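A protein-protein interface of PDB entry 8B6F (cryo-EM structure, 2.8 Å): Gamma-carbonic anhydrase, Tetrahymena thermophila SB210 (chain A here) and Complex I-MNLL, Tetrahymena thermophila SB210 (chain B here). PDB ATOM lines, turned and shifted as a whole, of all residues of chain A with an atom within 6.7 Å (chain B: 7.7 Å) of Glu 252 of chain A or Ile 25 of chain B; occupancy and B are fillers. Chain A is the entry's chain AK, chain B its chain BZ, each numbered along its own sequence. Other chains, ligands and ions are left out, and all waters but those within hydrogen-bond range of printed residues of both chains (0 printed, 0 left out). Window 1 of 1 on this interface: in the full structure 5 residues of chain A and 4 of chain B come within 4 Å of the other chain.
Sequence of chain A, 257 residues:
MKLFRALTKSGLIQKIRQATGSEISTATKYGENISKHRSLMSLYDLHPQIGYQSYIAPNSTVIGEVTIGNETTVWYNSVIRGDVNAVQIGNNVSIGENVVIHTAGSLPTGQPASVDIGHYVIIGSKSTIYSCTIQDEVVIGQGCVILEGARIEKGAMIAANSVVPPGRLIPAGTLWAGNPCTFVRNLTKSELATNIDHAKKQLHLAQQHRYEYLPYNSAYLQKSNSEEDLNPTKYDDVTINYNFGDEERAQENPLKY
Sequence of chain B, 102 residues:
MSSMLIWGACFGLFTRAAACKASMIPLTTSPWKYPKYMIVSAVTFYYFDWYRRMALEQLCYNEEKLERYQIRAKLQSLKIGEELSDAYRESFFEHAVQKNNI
NH2 of Arg 210 of chain A is in salt-bridge range of OE2 of Glu 252 of chain A, 2.8 Å away. The side-chain hydroxyl of Thr 29 of chain B is in hydrogen-bond range of the backbone carbonyl oxygen of Pro 26 of chain B, 2.9 Å away. N of Ile 25 of chain B lies within hydrogen-bond range of O of Cys 20 of chain B (3.1 Å). The side-chain hydroxyl (OG) of Ser 23 of chain B lies within hydrogen-bond range of the backbone carbonyl oxygen (O) of Ala 19 of chain B. OE2 of Glu 252 of chain A sits at hydrogen-bond distance from N of Gln 53 of chain A (2.6 Å). NH2 of Arg 16 of chain B lies within hydrogen-bond range of O of Thr 29 of chain B (2.5 Å).
Met 24 of chain B touches Tyr 52 of chain A (CE to CB, 3.8 Å). Gln 53 of chain A touches Met 24 of chain B. Ala 250 of chain A touches Ser 23 of chain B. Gln 251 of chain A touches Ile 25 of chain B. Gln 251 of chain A touches Thr 29 of chain B. Glu 252 of chain A touches Met 24 of chain B. CG2 of Ile 25 of chain B touches N of Glu 252 of chain A, at 3.6 Å.
Printed residues of chain B within 4 Å of Tyr 52 of chain A: Met 24. Of the printed residues of chain B, Gln 53 of chain A touches Met 24 (3.5 Å). Of the printed residues of chain B, Gln 251 of chain A touches Ile 25 (3.3 Å) and Thr 29 (3.8 Å). Of the printed residues of chain A, Met 24 of chain B touches Tyr 52, Gln 53 and Glu 252. Ile 25 of chain B touches two residues of chain A. Of the printed residues of chain A, Thr 29 of chain B touches Gln 251 (3.8 Å). The nearest residue of chain A that does not touch Ile 25 of chain B is Ala 250 of chain A (4.1 Å). The nearest printed residue of chain A that does not touch Ser 23 of chain B is Glu 252 of chain A (4.02 Å).
Of the 13 printed residues of chain A, 5 touch a printed residue of chain B. Of the 15 printed residues of chain B, 4 touch a printed residue of chain A. Hydrophobic or aromatic side chains of chain B within 4 Å of the printed part of chain A: Met 24 and Ile 25. Along chain B the printed residues that touch a printed residue of chain A span positions 23 to 29. Among the printed residues, no Asp or Glu carboxylate lies within 4 Å of a Lys or Arg side-chain nitrogen of the other chain.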
ATOM      1  N   ILE A  50      17.346   0.548 -12.928  1.00  0.00           N
ATOM      2  CA  ILE A  50      16.449  -0.250 -13.755  1.00  0.00           C
ATOM      3  C   ILE A  50      15.022  -0.020 -13.280  1.00  0.00           C
ATOM      4  O   ILE A  50      14.755  -0.032 -12.074  1.00  0.00           O
ATOM      5  CB  ILE A  50      16.809  -1.749 -13.709  1.00  0.00           C
ATOM      6  CG1 ILE A  50      18.194  -1.989 -14.313  1.00  0.00           C
ATOM      7  CG2 ILE A  50      15.780  -2.581 -14.455  1.00  0.00           C
ATOM      8  CD1 ILE A  50      19.322  -1.919 -13.316  1.00  0.00           C
ATOM      9  N   GLY A  51      14.111   0.187 -14.228  1.00  0.00           N
ATOM     10  CA  GLY A  51      12.718   0.420 -13.920  1.00  0.00           C
ATOM     11  C   GLY A  51      11.961  -0.871 -13.663  1.00  0.00           C
ATOM     12  O   GLY A  51      12.524  -1.966 -13.609  1.00  0.00           O
ATOM     13  N   TYR A  52      10.650  -0.728 -13.506  1.00  0.00           N
ATOM     14  CA  TYR A  52       9.801  -1.866 -13.190  1.00  0.00           C
ATOM     15  C   TYR A  52       9.548  -2.719 -14.426  1.00  0.00           C
ATOM     16  O   TYR A  52       9.513  -2.224 -15.555  1.00  0.00           O
ATOM     17  CB  TYR A  52       8.470  -1.402 -12.595  1.00  0.00           C
ATOM     18  CG  TYR A  52       7.558  -0.676 -13.558  1.00  0.00           C
ATOM     19  CD1 TYR A  52       6.736  -1.376 -14.432  1.00  0.00           C
ATOM     20  CD2 TYR A  52       7.495   0.710 -13.570  1.00  0.00           C
ATOM     21  CE1 TYR A  52       5.893  -0.718 -15.304  1.00  0.00           C
ATOM     22  CE2 TYR A  52       6.654   1.377 -14.438  1.00  0.00           C
ATOM     23  CZ  TYR A  52       5.856   0.658 -15.303  1.00  0.00           C
ATOM     24  OH  TYR A  52       5.017   1.321 -16.169  1.00  0.00           O
ATOM     25  N   GLN A  53       9.375  -4.020 -14.199  1.00  0.00           N
ATOM     26  CA  GLN A  53       9.095  -4.988 -15.256  1.00  0.00           C
ATOM     27  C   GLN A  53      10.203  -5.043 -16.297  1.00  0.00           C
ATOM     28  O   GLN A  53       9.976  -5.490 -17.425  1.00  0.00           O
ATOM     29  CB  GLN A  53       7.751  -4.695 -15.932  1.00  0.00           C
ATOM     30  CG  GLN A  53       6.549  -4.914 -15.027  1.00  0.00           C
ATOM     31  CD  GLN A  53       6.371  -6.367 -14.640  1.00  0.00           C
ATOM     32  OE1 GLN A  53       6.388  -7.252 -15.492  1.00  0.00           O
ATOM     33  NE2 GLN A  53       6.207  -6.620 -13.347  1.00  0.00           N
ATOM     34  N   SER A  54      11.405  -4.601 -15.941  1.00  0.00           N
ATOM     35  CA  SER A  54      12.558  -4.650 -16.829  1.00  0.00           C
ATOM     36  C   SER A  54      13.387  -5.880 -16.484  1.00  0.00           C
ATOM     37  O   SER A  54      13.815  -6.042 -15.338  1.00  0.00           O
ATOM     38  CB  SER A  54      13.402  -3.383 -16.698  1.00  0.00           C
ATOM     39  OG  SER A  54      12.707  -2.252 -17.193  1.00  0.00           O
ATOM     40  N   ARG A 210      10.899 -14.012 -16.939  1.00  0.00           N
ATOM     41  CA  ARG A 210      11.041 -13.510 -15.577  1.00  0.00           C
ATOM     42  C   ARG A 210      10.418 -14.461 -14.564  1.00  0.00           C
ATOM     43  O   ARG A 210      10.978 -14.688 -13.486  1.00  0.00           O
ATOM     44  CB  ARG A 210      10.394 -12.127 -15.486  1.00  0.00           C
ATOM     45  CG  ARG A 210      10.536 -11.428 -14.148  1.00  0.00           C
ATOM     46  CD  ARG A 210       9.461 -10.361 -14.000  1.00  0.00           C
ATOM     47  NE  ARG A 210       9.905  -9.231 -13.194  1.00  0.00           N
ATOM     48  CZ  ARG A 210      10.568  -8.186 -13.667  1.00  0.00           C
ATOM     49  NH1 ARG A 210      10.904  -8.099 -14.944  1.00  0.00           N
ATOM     50  NH2 ARG A 210      10.908  -7.204 -12.838  1.00  0.00           N
ATOM     51  N   ARG A 249       9.479  -4.318   1.337  1.00  0.00           N
ATOM     52  CA  ARG A 249       9.656  -4.089  -0.090  1.00  0.00           C
ATOM     53  C   ARG A 249       9.095  -5.262  -0.884  1.00  0.00           C
ATOM     54  O   ARG A 249       9.199  -6.420  -0.470  1.00  0.00           O
ATOM     55  CB  ARG A 249      11.135  -3.893  -0.412  1.00  0.00           C
ATOM     56  CG  ARG A 249      11.422  -3.629  -1.879  1.00  0.00           C
ATOM     57  CD  ARG A 249      12.897  -3.360  -2.101  1.00  0.00           C
ATOM     58  NE  ARG A 249      13.208  -3.142  -3.507  1.00  0.00           N
ATOM     59  CZ  ARG A 249      14.410  -2.824  -3.964  1.00  0.00           C
ATOM     60  NH1 ARG A 249      15.441  -2.669  -3.151  1.00  0.00           N
ATOM     61  NH2 ARG A 249      14.584  -2.654  -5.271  1.00  0.00           N
ATOM     62  N   ALA A 250       8.495  -4.957  -2.029  1.00  0.00           N
ATOM     63  CA  ALA A 250       7.920  -5.988  -2.877  1.00  0.00           C
ATOM     64  C   ALA A 250       8.990  -6.613  -3.760  1.00  0.00           C
ATOM     65  O   ALA A 250       9.851  -5.916  -4.304  1.00  0.00           O
ATOM     66  CB  ALA A 250       6.805  -5.405  -3.743  1.00  0.00           C
ATOM     67  N   GLN A 251       8.930  -7.937  -3.905  1.00  0.00           N
ATOM     68  CA  GLN A 251       9.861  -8.666  -4.764  1.00  0.00           C
ATOM     69  C   GLN A 251       9.427  -8.548  -6.228  1.00  0.00           C
ATOM     70  O   GLN A 251       9.133  -9.529  -6.909  1.00  0.00           O
ATOM     71  CB  GLN A 251       9.956 -10.124  -4.337  1.00  0.00           C
ATOM     72  CG  GLN A 251      10.420 -10.336  -2.907  1.00  0.00           C
ATOM     73  CD  GLN A 251       9.290 -10.247  -1.904  1.00  0.00           C
ATOM     74  OE1 GLN A 251       8.179  -9.834  -2.234  1.00  0.00           O
ATOM     75  NE2 GLN A 251       9.568 -10.644  -0.669  1.00  0.00           N
ATOM     76  N   GLU A 252       9.397  -7.305  -6.706  1.00  0.00           N
ATOM     77  CA  GLU A 252       8.932  -7.049  -8.063  1.00  0.00           C
ATOM     78  C   GLU A 252       9.828  -7.729  -9.089  1.00  0.00           C
ATOM     79  O   GLU A 252       9.337  -8.330 -10.050  1.00  0.00           O
ATOM     80  CB  GLU A 252       8.861  -5.541  -8.308  1.00  0.00           C
ATOM     81  CG  GLU A 252       8.305  -5.149  -9.669  1.00  0.00           C
ATOM     82  CD  GLU A 252       9.381  -4.971 -10.724  1.00  0.00           C
ATOM     83  OE1 GLU A 252      10.511  -4.574 -10.369  1.00  0.00           O
ATOM     84  OE2 GLU A 252       9.093  -5.223 -11.912  1.00  0.00           O
ATOM     85  N   ASN A 253      11.143  -7.650  -8.900  1.00  0.00           N
ATOM     86  CA  ASN A 253      12.094  -8.270  -9.816  1.00  0.00           C
ATOM     87  C   ASN A 253      12.789  -9.429  -9.117  1.00  0.00           C
ATOM     88  O   ASN A 253      13.521  -9.203  -8.141  1.00  0.00           O
ATOM     89  CB  ASN A 253      13.122  -7.246 -10.297  1.00  0.00           C
ATOM     90  CG  ASN A 253      13.881  -7.720 -11.516  1.00  0.00           C
ATOM     91  OD1 ASN A 253      13.440  -7.527 -12.646  1.00  0.00           O
ATOM     92  ND2 ASN A 253      15.028  -8.343 -11.294  1.00  0.00           N
ATOM     93  N   PRO A 254      12.595 -10.677  -9.556  1.00  0.00           N
ATOM     94  CA  PRO A 254      13.260 -11.793  -8.864  1.00  0.00           C
ATOM     95  C   PRO A 254      14.776 -11.709  -8.891  1.00  0.00           C
ATOM     96  O   PRO A 254      15.427 -12.173  -7.948  1.00  0.00           O
ATOM     97  CB  PRO A 254      12.743 -13.027  -9.617  1.00  0.00           C
ATOM     98  CG  PRO A 254      12.343 -12.525 -10.947  1.00  0.00           C
ATOM     99  CD  PRO A 254      11.833 -11.137 -10.729  1.00  0.00           C
ATOM    100  N   LEU A 255      15.359 -11.135  -9.940  1.00  0.00           N
ATOM    101  CA  LEU A 255      16.813 -11.049 -10.073  1.00  0.00           C
ATOM    102  C   LEU A 255      17.371  -9.829  -9.348  1.00  0.00           C
ATOM    103  O   LEU A 255      18.108  -9.026  -9.916  1.00  0.00           O
ATOM    104  CB  LEU A 255      17.194 -11.022 -11.548  1.00  0.00           C
ATOM    105  CG  LEU A 255      16.644 -12.158 -12.409  1.00  0.00           C
ATOM    106  CD1 LEU A 255      17.033 -11.953 -13.861  1.00  0.00           C
ATOM    107  CD2 LEU A 255      17.136 -13.501 -11.909  1.00  0.00           C
ATOM    108  N   ARG B  16      -5.171  -9.932  -0.258  1.00  0.00           N
ATOM    109  CA  ARG B  16      -3.835 -10.436  -0.557  1.00  0.00           C
ATOM    110  C   ARG B  16      -3.620 -10.557  -2.060  1.00  0.00           C
ATOM    111  O   ARG B  16      -2.567 -10.171  -2.578  1.00  0.00           O
ATOM    112  CB  ARG B  16      -3.621 -11.785   0.130  1.00  0.00           C
ATOM    113  CG  ARG B  16      -2.328 -12.490  -0.254  1.00  0.00           C
ATOM    114  CD  ARG B  16      -1.096 -11.687   0.134  1.00  0.00           C
ATOM    115  NE  ARG B  16       0.091 -12.171  -0.557  1.00  0.00           N
ATOM    116  CZ  ARG B  16       1.305 -11.658  -0.412  1.00  0.00           C
ATOM    117  NH1 ARG B  16       1.537 -10.659   0.421  1.00  0.00           N
ATOM    118  NH2 ARG B  16       2.310 -12.158  -1.124  1.00  0.00           N
ATOM    119  N   ALA B  17      -4.606 -11.098  -2.778  1.00  0.00           N
ATOM    120  CA  ALA B  17      -4.476 -11.226  -4.225  1.00  0.00           C
ATOM    121  C   ALA B  17      -4.325  -9.861  -4.882  1.00  0.00           C
ATOM    122  O   ALA B  17      -3.493  -9.681  -5.776  1.00  0.00           O
ATOM    123  CB  ALA B  17      -5.685 -11.965  -4.797  1.00  0.00           C
ATOM    124  N   ALA B  19      -3.181  -7.116  -3.494  1.00  0.00           N
ATOM    125  CA  ALA B  19      -1.871  -6.576  -3.147  1.00  0.00           C
ATOM    126  C   ALA B  19      -0.786  -7.161  -4.036  1.00  0.00           C
ATOM    127  O   ALA B  19       0.108  -6.440  -4.492  1.00  0.00           O
ATOM    128  CB  ALA B  19      -1.570  -6.841  -1.673  1.00  0.00           C
ATOM    129  N   CYS B  20      -0.833  -8.470  -4.282  1.00  0.00           N
ATOM    130  CA  CYS B  20       0.138  -9.076  -5.184  1.00  0.00           C
ATOM    131  C   CYS B  20       0.029  -8.474  -6.579  1.00  0.00           C
ATOM    132  O   CYS B  20       1.040  -8.135  -7.203  1.00  0.00           O
ATOM    133  CB  CYS B  20      -0.067 -10.589  -5.226  1.00  0.00           C
ATOM    134  SG  CYS B  20       0.369 -11.432  -3.690  1.00  0.00           S
ATOM    135  N   LYS B  21      -1.199  -8.334  -7.088  1.00  0.00           N
ATOM    136  CA  LYS B  21      -1.383  -7.781  -8.427  1.00  0.00           C
ATOM    137  C   LYS B  21      -0.886  -6.345  -8.509  1.00  0.00           C
ATOM    138  O   LYS B  21      -0.233  -5.960  -9.485  1.00  0.00           O
ATOM    139  CB  LYS B  21      -2.857  -7.854  -8.831  1.00  0.00           C
ATOM    140  CG  LYS B  21      -3.365  -9.271  -9.053  1.00  0.00           C
ATOM    141  CD  LYS B  21      -4.842  -9.293  -9.428  1.00  0.00           C
ATOM    142  CE  LYS B  21      -5.098  -8.675 -10.792  1.00  0.00           C
ATOM    143  NZ  LYS B  21      -4.341  -9.363 -11.872  1.00  0.00           N
ATOM    144  N   ALA B  22      -1.193  -5.534  -7.495  1.00  0.00           N
ATOM    145  CA  ALA B  22      -0.759  -4.142  -7.503  1.00  0.00           C
ATOM    146  C   ALA B  22       0.758  -4.033  -7.436  1.00  0.00           C
ATOM    147  O   ALA B  22       1.357  -3.196  -8.119  1.00  0.00           O
ATOM    148  CB  ALA B  22      -1.399  -3.391  -6.338  1.00  0.00           C
ATOM    149  N   SER B  23       1.396  -4.860  -6.607  1.00  0.00           N
ATOM    150  CA  SER B  23       2.848  -4.867  -6.518  1.00  0.00           C
ATOM    151  C   SER B  23       3.507  -5.528  -7.718  1.00  0.00           C
ATOM    152  O   SER B  23       4.733  -5.453  -7.846  1.00  0.00           O
ATOM    153  CB  SER B  23       3.291  -5.577  -5.238  1.00  0.00           C
ATOM    154  OG  SER B  23       2.782  -4.925  -4.089  1.00  0.00           O
ATOM    155  N   MET B  24       2.732  -6.172  -8.590  1.00  0.00           N
ATOM    156  CA  MET B  24       3.234  -6.829  -9.791  1.00  0.00           C
ATOM    157  C   MET B  24       4.097  -8.039  -9.466  1.00  0.00           C
ATOM    158  O   MET B  24       4.924  -8.452 -10.283  1.00  0.00           O
ATOM    159  CB  MET B  24       4.021  -5.854 -10.673  1.00  0.00           C
ATOM    160  CG  MET B  24       3.208  -4.657 -11.141  1.00  0.00           C
ATOM    161  SD  MET B  24       4.142  -3.540 -12.202  1.00  0.00           S
ATOM    162  CE  MET B  24       5.384  -2.948 -11.059  1.00  0.00           C
ATOM    163  N   ILE B  25       3.919  -8.617  -8.284  1.00  0.00           N
ATOM    164  CA  ILE B  25       4.627  -9.833  -7.894  1.00  0.00           C
ATOM    165  C   ILE B  25       3.704 -11.020  -8.150  1.00  0.00           C
ATOM    166  O   ILE B  25       2.477 -10.850  -8.167  1.00  0.00           O
ATOM    167  CB  ILE B  25       5.073  -9.773  -6.424  1.00  0.00           C
ATOM    168  CG1 ILE B  25       3.862  -9.607  -5.498  1.00  0.00           C
ATOM    169  CG2 ILE B  25       6.050  -8.628  -6.233  1.00  0.00           C
ATOM    170  CD1 ILE B  25       4.203  -9.582  -4.022  1.00  0.00           C
ATOM    171  N   PRO B  26       4.233 -12.225  -8.355  1.00  0.00           N
ATOM    172  CA  PRO B  26       3.351 -13.377  -8.573  1.00  0.00           C
ATOM    173  C   PRO B  26       2.424 -13.592  -7.388  1.00  0.00           C
ATOM    174  O   PRO B  26       2.784 -13.348  -6.236  1.00  0.00           O
ATOM    175  CB  PRO B  26       4.328 -14.547  -8.744  1.00  0.00           C
ATOM    176  CG  PRO B  26       5.603 -13.919  -9.162  1.00  0.00           C
ATOM    177  CD  PRO B  26       5.653 -12.594  -8.470  1.00  0.00           C
ATOM    178  N   LEU B  27       1.212 -14.058  -7.686  1.00  0.00           N
ATOM    179  CA  LEU B  27       0.214 -14.272  -6.644  1.00  0.00           C
ATOM    180  C   LEU B  27       0.614 -15.363  -5.662  1.00  0.00           C
ATOM    181  O   LEU B  27      -0.007 -15.468  -4.599  1.00  0.00           O
ATOM    182  CB  LEU B  27      -1.141 -14.613  -7.270  1.00  0.00           C
ATOM    183  CG  LEU B  27      -1.932 -13.442  -7.865  1.00  0.00           C
ATOM    184  CD1 LEU B  27      -1.216 -12.820  -9.054  1.00  0.00           C
ATOM    185  CD2 LEU B  27      -3.331 -13.883  -8.261  1.00  0.00           C
ATOM    186  N   THR B  28       1.624 -16.166  -5.983  1.00  0.00           N
ATOM    187  CA  THR B  28       2.118 -17.209  -5.096  1.00  0.00           C
ATOM    188  C   THR B  28       3.262 -16.735  -4.208  1.00  0.00           C
ATOM    189  O   THR B  28       3.848 -17.549  -3.488  1.00  0.00           O
ATOM    190  CB  THR B  28       2.567 -18.425  -5.911  1.00  0.00           C
ATOM    191  OG1 THR B  28       3.531 -18.024  -6.892  1.00  0.00           O
ATOM    192  CG2 THR B  28       1.382 -19.070  -6.601  1.00  0.00           C
ATOM    193  N   THR B  29       3.603 -15.451  -4.254  1.00  0.00           N
ATOM    194  CA  THR B  29       4.671 -14.929  -3.411  1.00  0.00           C
ATOM    195  C   THR B  29       4.201 -14.817  -1.966  1.00  0.00           C
ATOM    196  O   THR B  29       3.047 -14.478  -1.695  1.00  0.00           O
ATOM    197  CB  THR B  29       5.129 -13.562  -3.920  1.00  0.00           C
ATOM    198  OG1 THR B  29       5.533 -13.666  -5.291  1.00  0.00           O
ATOM    199  CG2 THR B  29       6.298 -13.040  -3.097  1.00  0.00           C
ATOM    200  N   SER B  30       5.109 -15.101  -1.037  1.00  0.00           N
ATOM    201  CA  SER B  30       4.825 -15.071   0.393  1.00  0.00           C
ATOM    202  C   SER B  30       3.526 -15.816   0.712  1.00  0.00           C
ATOM    203  O   SER B  30       2.575 -15.224   1.230  1.00  0.00           O
ATOM    204  CB  SER B  30       4.759 -13.638   0.902  1.00  0.00           C
ATOM    205  OG  SER B  30       5.987 -12.960   0.694  1.00  0.00           O
ATOM    206  N   LYS B  33       1.316 -15.451   3.924  1.00  0.00           N
ATOM    207  CA  LYS B  33       0.514 -14.263   4.182  1.00  0.00           C
ATOM    208  C   LYS B  33      -0.956 -14.460   3.843  1.00  0.00           C
ATOM    209  O   LYS B  33      -1.792 -13.677   4.307  1.00  0.00           O
ATOM    210  CB  LYS B  33       1.070 -13.074   3.399  1.00  0.00           C
ATOM    211  CG  LYS B  33       2.322 -12.471   4.021  1.00  0.00           C
ATOM    212  CD  LYS B  33       2.876 -11.338   3.176  1.00  0.00           C
ATOM    213  CE  LYS B  33       3.940 -10.555   3.930  1.00  0.00           C
ATOM    214  NZ  LYS B  33       5.017 -11.431   4.463  1.00  0.00           N
